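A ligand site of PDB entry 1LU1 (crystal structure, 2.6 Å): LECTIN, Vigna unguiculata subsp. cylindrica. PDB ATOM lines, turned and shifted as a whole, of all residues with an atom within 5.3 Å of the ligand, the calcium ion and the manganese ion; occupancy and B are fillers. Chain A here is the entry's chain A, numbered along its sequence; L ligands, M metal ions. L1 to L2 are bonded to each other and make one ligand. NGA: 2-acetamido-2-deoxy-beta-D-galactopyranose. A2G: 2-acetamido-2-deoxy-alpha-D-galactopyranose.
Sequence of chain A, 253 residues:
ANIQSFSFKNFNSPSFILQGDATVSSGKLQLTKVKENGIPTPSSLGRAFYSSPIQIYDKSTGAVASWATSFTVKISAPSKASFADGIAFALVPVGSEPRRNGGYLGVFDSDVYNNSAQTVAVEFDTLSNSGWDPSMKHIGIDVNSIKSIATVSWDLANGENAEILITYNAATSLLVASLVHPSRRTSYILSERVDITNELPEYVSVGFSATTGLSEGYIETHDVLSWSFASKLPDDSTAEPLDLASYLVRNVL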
ATOM      1  N   ALA A  84     -11.172   6.441 -19.089  1.00  0.00           N
ATOM      2  CA  ALA A  84     -10.764   5.902 -20.389  1.00  0.00           C
ATOM      3  C   ALA A  84     -11.499   4.573 -20.558  1.00  0.00           C
ATOM      4  O   ALA A  84     -11.686   3.845 -19.573  1.00  0.00           O
ATOM      5  CB  ALA A  84      -9.274   5.683 -20.430  1.00  0.00           C
ATOM      6  N   ASP A  85     -11.928   4.242 -21.771  1.00  0.00           N
ATOM      7  CA  ASP A  85     -11.761   5.072 -22.956  1.00  0.00           C
ATOM      8  C   ASP A  85     -13.078   5.590 -23.504  1.00  0.00           C
ATOM      9  O   ASP A  85     -13.108   6.563 -24.240  1.00  0.00           O
ATOM     10  CB  ASP A  85     -11.046   4.274 -24.055  1.00  0.00           C
ATOM     11  CG  ASP A  85      -9.620   4.740 -24.279  1.00  0.00           C
ATOM     12  OD1 ASP A  85      -9.444   5.890 -24.718  1.00  0.00           O
ATOM     13  OD2 ASP A  85      -8.693   3.942 -24.009  1.00  0.00           O
ATOM     14  N   ASN A 101      -8.613  -1.860 -30.111  1.00  0.00           N
ATOM     15  CA  ASN A 101      -9.004  -1.538 -28.740  1.00  0.00           C
ATOM     16  C   ASN A 101      -8.527  -0.137 -28.347  1.00  0.00           C
ATOM     17  O   ASN A 101      -8.100   0.644 -29.197  1.00  0.00           O
ATOM     18  CB  ASN A 101      -8.461  -2.574 -27.749  1.00  0.00           C
ATOM     19  CG  ASN A 101      -6.928  -2.749 -27.827  1.00  0.00           C
ATOM     20  OD1 ASN A 101      -6.341  -3.442 -27.005  1.00  0.00           O
ATOM     21  ND2 ASN A 101      -6.319  -2.120 -28.813  1.00  0.00           N
ATOM     22  N   GLY A 102      -8.608   0.188 -27.062  1.00  0.00           N
ATOM     23  CA  GLY A 102      -8.182   1.502 -26.620  1.00  0.00           C
ATOM     24  C   GLY A 102      -9.043   2.636 -27.150  1.00  0.00           C
ATOM     25  O   GLY A 102     -10.278   2.562 -27.116  1.00  0.00           O
ATOM     26  N   GLY A 103      -8.391   3.675 -27.649  1.00  0.00           N
ATOM     27  CA  GLY A 103      -9.099   4.837 -28.168  1.00  0.00           C
ATOM     28  C   GLY A 103      -9.939   4.608 -29.401  1.00  0.00           C
ATOM     29  O   GLY A 103     -10.581   5.545 -29.891  1.00  0.00           O
ATOM     30  N   TYR A 104      -9.939   3.392 -29.923  1.00  0.00           N
ATOM     31  CA  TYR A 104     -10.739   3.087 -31.111  1.00  0.00           C
ATOM     32  C   TYR A 104     -12.090   2.510 -30.708  1.00  0.00           C
ATOM     33  O   TYR A 104     -12.927   2.192 -31.554  1.00  0.00           O
ATOM     34  CB  TYR A 104      -9.973   2.121 -32.028  1.00  0.00           C
ATOM     35  CG  TYR A 104      -8.807   2.795 -32.709  1.00  0.00           C
ATOM     36  CD1 TYR A 104      -9.001   3.551 -33.856  1.00  0.00           C
ATOM     37  CD2 TYR A 104      -7.517   2.720 -32.170  1.00  0.00           C
ATOM     38  CE1 TYR A 104      -7.951   4.227 -34.470  1.00  0.00           C
ATOM     39  CE2 TYR A 104      -6.448   3.386 -32.780  1.00  0.00           C
ATOM     40  CZ  TYR A 104      -6.672   4.141 -33.932  1.00  0.00           C
ATOM     41  OH  TYR A 104      -5.631   4.804 -34.534  1.00  0.00           O
ATOM     42  N   GLU A 123     -20.446   8.161 -30.152  1.00  0.00           N
ATOM     43  CA  GLU A 123     -19.551   7.857 -29.056  1.00  0.00           C
ATOM     44  C   GLU A 123     -19.627   8.822 -27.904  1.00  0.00           C
ATOM     45  O   GLU A 123     -19.931  10.011 -28.067  1.00  0.00           O
ATOM     46  CB  GLU A 123     -18.113   7.842 -29.541  1.00  0.00           C
ATOM     47  CG  GLU A 123     -17.756   9.112 -30.263  1.00  0.00           C
ATOM     48  CD  GLU A 123     -16.284   9.413 -30.237  1.00  0.00           C
ATOM     49  OE1 GLU A 123     -15.534   8.841 -31.060  1.00  0.00           O
ATOM     50  OE2 GLU A 123     -15.868  10.222 -29.383  1.00  0.00           O
ATOM     51  N   ASP A 125     -16.952   9.588 -25.603  1.00  0.00           N
ATOM     52  CA  ASP A 125     -15.512   9.576 -25.417  1.00  0.00           C
ATOM     53  C   ASP A 125     -15.042  10.175 -24.092  1.00  0.00           C
ATOM     54  O   ASP A 125     -15.148  11.381 -23.907  1.00  0.00           O
ATOM     55  CB  ASP A 125     -14.904  10.361 -26.563  1.00  0.00           C
ATOM     56  CG  ASP A 125     -13.525   9.905 -26.915  1.00  0.00           C
ATOM     57  OD1 ASP A 125     -12.828   9.398 -26.006  1.00  0.00           O
ATOM     58  OD2 ASP A 125     -13.138  10.077 -28.089  1.00  0.00           O
ATOM     59  N   LEU A 127     -11.822  10.038 -22.947  1.00  0.00           N
ATOM     60  CA  LEU A 127     -10.380  10.308 -22.978  1.00  0.00           C
ATOM     61  C   LEU A 127      -9.990  10.929 -24.315  1.00  0.00           C
ATOM     62  O   LEU A 127     -10.224  10.358 -25.388  1.00  0.00           O
ATOM     63  CB  LEU A 127      -9.568   9.035 -22.754  1.00  0.00           C
ATOM     64  CG  LEU A 127      -8.052   9.263 -22.779  1.00  0.00           C
ATOM     65  CD1 LEU A 127      -7.518   9.309 -21.356  1.00  0.00           C
ATOM     66  CD2 LEU A 127      -7.376   8.174 -23.566  1.00  0.00           C
ATOM     67  N   SER A 128      -9.378  12.107 -24.239  1.00  0.00           N
ATOM     68  CA  SER A 128      -8.966  12.840 -25.420  1.00  0.00           C
ATOM     69  C   SER A 128      -7.680  12.292 -26.042  1.00  0.00           C
ATOM     70  O   SER A 128      -6.621  12.337 -25.436  1.00  0.00           O
ATOM     71  CB  SER A 128      -8.769  14.307 -25.057  1.00  0.00           C
ATOM     72  OG  SER A 128      -8.777  15.105 -26.222  1.00  0.00           O
ATOM     73  N   ASN A 129      -7.785  11.791 -27.275  1.00  0.00           N
ATOM     74  CA  ASN A 129      -6.624  11.268 -27.977  1.00  0.00           C
ATOM     75  C   ASN A 129      -6.094  12.366 -28.898  1.00  0.00           C
ATOM     76  O   ASN A 129      -6.692  12.671 -29.927  1.00  0.00           O
ATOM     77  CB  ASN A 129      -7.007  10.049 -28.814  1.00  0.00           C
ATOM     78  CG  ASN A 129      -7.633   8.949 -27.982  1.00  0.00           C
ATOM     79  OD1 ASN A 129      -8.858   8.798 -27.960  1.00  0.00           O
ATOM     80  ND2 ASN A 129      -6.803   8.175 -27.306  1.00  0.00           N
ATOM     81  N   SER A 130      -4.963  12.955 -28.518  1.00  0.00           N
ATOM     82  CA  SER A 130      -4.321  14.042 -29.253  1.00  0.00           C
ATOM     83  C   SER A 130      -4.406  14.037 -30.785  1.00  0.00           C
ATOM     84  O   SER A 130      -4.465  15.107 -31.401  1.00  0.00           O
ATOM     85  CB  SER A 130      -2.848  14.121 -28.858  1.00  0.00           C
ATOM     86  OG  SER A 130      -2.445  12.933 -28.207  1.00  0.00           O
ATOM     87  N   TRP A 132      -6.912  13.024 -32.872  1.00  0.00           N
ATOM     88  CA  TRP A 132      -8.200  13.276 -33.530  1.00  0.00           C
ATOM     89  C   TRP A 132      -9.298  13.748 -32.590  1.00  0.00           C
ATOM     90  O   TRP A 132     -10.404  14.026 -33.036  1.00  0.00           O
ATOM     91  CB  TRP A 132      -8.690  11.993 -34.200  1.00  0.00           C
ATOM     92  CG  TRP A 132      -8.884  10.876 -33.205  1.00  0.00           C
ATOM     93  CD1 TRP A 132      -9.895  10.755 -32.296  1.00  0.00           C
ATOM     94  CD2 TRP A 132      -8.037   9.743 -33.017  1.00  0.00           C
ATOM     95  NE1 TRP A 132      -9.726   9.624 -31.534  1.00  0.00           N
ATOM     96  CE2 TRP A 132      -8.591   8.972 -31.966  1.00  0.00           C
ATOM     97  CE3 TRP A 132      -6.858   9.287 -33.631  1.00  0.00           C
ATOM     98  CZ2 TRP A 132      -8.011   7.794 -31.507  1.00  0.00           C
ATOM     99  CZ3 TRP A 132      -6.274   8.116 -33.178  1.00  0.00           C
ATOM    100  CH2 TRP A 132      -6.858   7.375 -32.133  1.00  0.00           C
ATOM    101  N   ASP A 133      -8.990  13.847 -31.306  1.00  0.00           N
ATOM    102  CA  ASP A 133     -10.000  14.237 -30.326  1.00  0.00           C
ATOM    103  C   ASP A 133      -9.988  15.696 -29.908  1.00  0.00           C
ATOM    104  O   ASP A 133      -8.946  16.355 -29.913  1.00  0.00           O
ATOM    105  CB  ASP A 133      -9.836  13.382 -29.062  1.00  0.00           C
ATOM    106  CG  ASP A 133     -10.705  12.145 -29.075  1.00  0.00           C
ATOM    107  OD1 ASP A 133     -11.533  12.030 -30.005  1.00  0.00           O
ATOM    108  OD2 ASP A 133     -10.556  11.294 -28.165  1.00  0.00           O
ATOM    109  N   PRO A 134     -11.162  16.217 -29.534  1.00  0.00           N
ATOM    110  CA  PRO A 134     -11.301  17.608 -29.085  1.00  0.00           C
ATOM    111  C   PRO A 134     -10.668  17.716 -27.706  1.00  0.00           C
ATOM    112  O   PRO A 134     -10.372  16.695 -27.094  1.00  0.00           O
ATOM    113  CB  PRO A 134     -12.818  17.821 -29.021  1.00  0.00           C
ATOM    114  CG  PRO A 134     -13.419  16.640 -29.725  1.00  0.00           C
ATOM    115  CD  PRO A 134     -12.459  15.529 -29.547  1.00  0.00           C
ATOM    116  N   HIS A 138     -16.252  14.265 -24.529  1.00  0.00           N
ATOM    117  CA  HIS A 138     -17.265  14.669 -25.483  1.00  0.00           C
ATOM    118  C   HIS A 138     -18.163  13.572 -26.044  1.00  0.00           C
ATOM    119  O   HIS A 138     -17.901  12.386 -25.892  1.00  0.00           O
ATOM    120  CB  HIS A 138     -16.555  15.301 -26.659  1.00  0.00           C
ATOM    121  CG  HIS A 138     -15.509  14.411 -27.272  1.00  0.00           C
ATOM    122  ND1 HIS A 138     -14.301  14.138 -26.679  1.00  0.00           N
ATOM    123  CD2 HIS A 138     -15.557  13.648 -28.389  1.00  0.00           C
ATOM    124  CE1 HIS A 138     -13.653  13.238 -27.441  1.00  0.00           C
ATOM    125  NE2 HIS A 138     -14.367  12.908 -28.496  1.00  0.00           N
ATOM    126  N   ASP A 142     -19.567   9.534 -35.206  1.00  0.00           N
ATOM    127  CA  ASP A 142     -18.517   8.942 -36.033  1.00  0.00           C
ATOM    128  C   ASP A 142     -19.055   8.223 -37.258  1.00  0.00           C
ATOM    129  O   ASP A 142     -19.857   7.304 -37.135  1.00  0.00           O
ATOM    130  CB  ASP A 142     -17.692   7.952 -35.219  1.00  0.00           C
ATOM    131  CG  ASP A 142     -17.152   8.552 -33.942  1.00  0.00           C
ATOM    132  OD1 ASP A 142     -16.966   9.787 -33.895  1.00  0.00           O
ATOM    133  OD2 ASP A 142     -16.932   7.792 -32.980  1.00  0.00           O
ATOM    134  N   ILE A 146     -12.669   7.148 -36.567  1.00  0.00           N
ATOM    135  CA  ILE A 146     -12.741   7.471 -35.145  1.00  0.00           C
ATOM    136  C   ILE A 146     -12.711   8.992 -34.910  1.00  0.00           C
ATOM    137  O   ILE A 146     -12.885   9.463 -33.781  1.00  0.00           O
ATOM    138  CB  ILE A 146     -11.612   6.775 -34.349  1.00  0.00           C
ATOM    139  CG1 ILE A 146     -11.931   6.818 -32.852  1.00  0.00           C
ATOM    140  CG2 ILE A 146     -10.268   7.429 -34.639  1.00  0.00           C
ATOM    141  CD1 ILE A 146     -13.105   5.930 -32.433  1.00  0.00           C
ATOM    142  N   SER A 148     -14.585  12.026 -35.078  1.00  0.00           N
ATOM    143  CA  SER A 148     -15.981  12.430 -35.196  1.00  0.00           C
ATOM    144  C   SER A 148     -16.188  13.576 -36.185  1.00  0.00           C
ATOM    145  O   SER A 148     -15.320  14.435 -36.327  1.00  0.00           O
ATOM    146  CB  SER A 148     -16.496  12.837 -33.803  1.00  0.00           C
ATOM    147  OG  SER A 148     -15.919  12.042 -32.787  1.00  0.00           O
ATOM    148  N   THR A 212     -11.609   0.060 -22.217  1.00  0.00           N
ATOM    149  CA  THR A 212     -10.962   0.776 -21.132  1.00  0.00           C
ATOM    150  C   THR A 212      -9.545   1.087 -21.617  1.00  0.00           C
ATOM    151  O   THR A 212      -9.105   0.541 -22.638  1.00  0.00           O
ATOM    152  CB  THR A 212     -10.924  -0.071 -19.849  1.00  0.00           C
ATOM    153  OG1 THR A 212     -10.339  -1.348 -20.114  1.00  0.00           O
ATOM    154  CG2 THR A 212     -12.321  -0.271 -19.310  1.00  0.00           C
ATOM    155  N   GLY A 213      -8.853   1.972 -20.910  1.00  0.00           N
ATOM    156  CA  GLY A 213      -7.508   2.386 -21.301  1.00  0.00           C
ATOM    157  C   GLY A 213      -6.432   1.332 -21.241  1.00  0.00           C
ATOM    158  O   GLY A 213      -6.548   0.351 -20.504  1.00  0.00           O
ATOM    159  N   LEU A 214      -5.371   1.538 -22.003  1.00  0.00           N
ATOM    160  CA  LEU A 214      -4.262   0.593 -22.080  1.00  0.00           C
ATOM    161  C   LEU A 214      -3.210   0.784 -21.002  1.00  0.00           C
ATOM    162  O   LEU A 214      -2.134   0.197 -21.072  1.00  0.00           O
ATOM    163  CB  LEU A 214      -3.607   0.681 -23.453  1.00  0.00           C
ATOM    164  CG  LEU A 214      -4.547   0.511 -24.644  1.00  0.00           C
ATOM    165  CD1 LEU A 214      -3.748   0.644 -25.944  1.00  0.00           C
ATOM    166  CD2 LEU A 214      -5.223  -0.857 -24.578  1.00  0.00           C
ATOM    167  N   SER A 215      -3.510   1.616 -20.012  1.00  0.00           N
ATOM    168  CA  SER A 215      -2.568   1.879 -18.916  1.00  0.00           C
ATOM    169  C   SER A 215      -3.153   1.485 -17.584  1.00  0.00           C
ATOM    170  O   SER A 215      -4.357   1.392 -17.433  1.00  0.00           O
ATOM    171  CB  SER A 215      -2.171   3.350 -18.887  1.00  0.00           C
ATOM    172  OG  SER A 215      -1.496   3.693 -20.077  1.00  0.00           O
ATOM    173  N   TYR A 218      -5.895   4.113 -16.256  1.00  0.00           N
ATOM    174  CA  TYR A 218      -6.927   4.673 -17.099  1.00  0.00           C
ATOM    175  C   TYR A 218      -8.050   3.676 -17.263  1.00  0.00           C
ATOM    176  O   TYR A 218      -8.113   2.967 -18.265  1.00  0.00           O
ATOM    177  CB  TYR A 218      -6.349   5.047 -18.443  1.00  0.00           C
ATOM    178  CG  TYR A 218      -5.452   6.242 -18.340  1.00  0.00           C
ATOM    179  CD1 TYR A 218      -4.134   6.102 -17.935  1.00  0.00           C
ATOM    180  CD2 TYR A 218      -5.923   7.508 -18.655  1.00  0.00           C
ATOM    181  CE1 TYR A 218      -3.288   7.203 -17.858  1.00  0.00           C
ATOM    182  CE2 TYR A 218      -5.089   8.611 -18.583  1.00  0.00           C
ATOM    183  CZ  TYR A 218      -3.775   8.459 -18.195  1.00  0.00           C
ATOM    184  OH  TYR A 218      -2.947   9.555 -18.169  1.00  0.00           O
HETATM  185  C1  NGA L   1       0.714   7.866 -24.722  1.00  0.00           C
HETATM  186  C2  NGA L   1      -0.785   7.655 -24.885  1.00  0.00           C
HETATM  187  C3  NGA L   1      -1.067   6.206 -25.172  1.00  0.00           C
HETATM  188  C4  NGA L   1      -0.199   5.608 -26.271  1.00  0.00           C
HETATM  189  C5  NGA L   1       1.257   5.946 -26.032  1.00  0.00           C
HETATM  190  C6  NGA L   1       2.192   5.475 -27.157  1.00  0.00           C
HETATM  191  C7  NGA L   1      -2.447   8.954 -23.767  1.00  0.00           C
HETATM  192  C8  NGA L   1      -3.111   9.332 -22.464  1.00  0.00           C
HETATM  193  N2  NGA L   1      -1.480   8.059 -23.676  1.00  0.00           N
HETATM  194  O1  NGA L   1       0.950   9.233 -24.677  1.00  0.00           O
HETATM  195  O3  NGA L   1      -2.452   6.072 -25.564  1.00  0.00           O
HETATM  196  O4  NGA L   1      -0.657   6.120 -27.516  1.00  0.00           O
HETATM  197  O5  NGA L   1       1.388   7.375 -25.877  1.00  0.00           O
HETATM  198  O7  NGA L   1      -2.829   9.427 -24.866  1.00  0.00           O
HETATM  199  O5  A2G L   2      -3.275   4.634 -23.771  1.00  0.00           O
HETATM  200  C1  A2G L   2      -3.122   4.855 -25.193  1.00  0.00           C
HETATM  201  C2  A2G L   2      -4.487   4.736 -25.904  1.00  0.00           C
HETATM  202  N2  A2G L   2      -4.341   5.107 -27.298  1.00  0.00           N
HETATM  203  C3  A2G L   2      -5.554   5.620 -25.247  1.00  0.00           C
HETATM  204  O3  A2G L   2      -6.806   5.422 -25.898  1.00  0.00           O
HETATM  205  C4  A2G L   2      -5.650   5.273 -23.757  1.00  0.00           C
HETATM  206  O4  A2G L   2      -6.017   3.906 -23.632  1.00  0.00           O
HETATM  207  C5  A2G L   2      -4.289   5.458 -23.125  1.00  0.00           C
HETATM  208  C6  A2G L   2      -4.302   5.082 -21.639  1.00  0.00           C
HETATM  209  O6  A2G L   2      -3.034   5.340 -21.078  1.00  0.00           O
HETATM  210  C7  A2G L   2      -4.943   4.386 -28.257  1.00  0.00           C
HETATM  211  O7  A2G L   2      -5.595   3.379 -28.005  1.00  0.00           O
HETATM  212  C8  A2G L   2      -4.791   4.840 -29.704  1.00  0.00           C
HETATM  213 CA    CA M   1     -10.831   9.055 -27.264  1.00  0.00          CA
HETATM  214 MN    MN M   2     -13.780  11.130 -30.197  1.00  0.00          MN
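ND2 of Asn 129 is in hydrogen-bond range of O3 of A2G L2 (3.1 Å). The side-chain carboxylate (OD2) of Asp 85 is in hydrogen-bond range of an oxygen (O4) of A2G L2, at 2.7 Å. N of Leu 214 lies within hydrogen-bond range of O4 of A2G L2 (2.9 Å). An oxygen (O6) of A2G L2 is in hydrogen-bond range of the side-chain hydroxyl (OG) of Ser 215 (2.5 Å). N of Gly 103 is in hydrogen-bond range of O7 of A2G L2 (2.8 Å).
The side-chain carboxylate (OD1) of Asp 142 lies within hydrogen-bond range of the side-chain hydroxyl (OG) of Ser 148 (2.7 Å). NE1 of Trp 132 lies close to OD1 of Asp 133. OD2 of Asp 142 lies close to OE1 of Glu 123 (2.6 Å). The backbone NH (N) of Gly 213 lies within hydrogen-bond range of the backbone carbonyl oxygen (O) of Tyr 218.
Residues that only touch the ligand: Gly 213 (3.2 Å), Tyr 218 (3.4 Å), Gly 102 (3.5 Å), Tyr 104 (3.8 Å) and Asn 101 (3.9 Å). Of the 24 residues printed, 11 come within 4 Å of the ligand.
The nearest printed residue that does not touch the calcium ion is Asp 85 (4.3 Å).
OG of Ser 148 touches the manganese ion, at 3.5 Å. Five residues have an atom within 4 Å of the manganese ion: Glu 123, Asp 125, Asp 133, His 138 and Ser 148. The nearest printed residue that does not touch the manganese ion is Ile 146 (4.1 Å).
The calcium ion is bound by OD1 of Asn 129 (2.1 Å), O of Leu 127 (2.4 Å), OD1 of Asp 125 (2.4 Å), OD2 of Asp 133 (2.4 Å) and OD2 of Asp 125 (2.7 Å).
The manganese ion is bound by the side-chain carboxylate (OE2) of Glu 123 (2.4 Å), the side-chain carboxylate (OD1) of Asp 133 (2.4 Å), the side-chain carboxylate (OD2) of Asp 125 (2.4 Å) and a ring nitrogen (NE2) of His 138 (2.5 Å).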
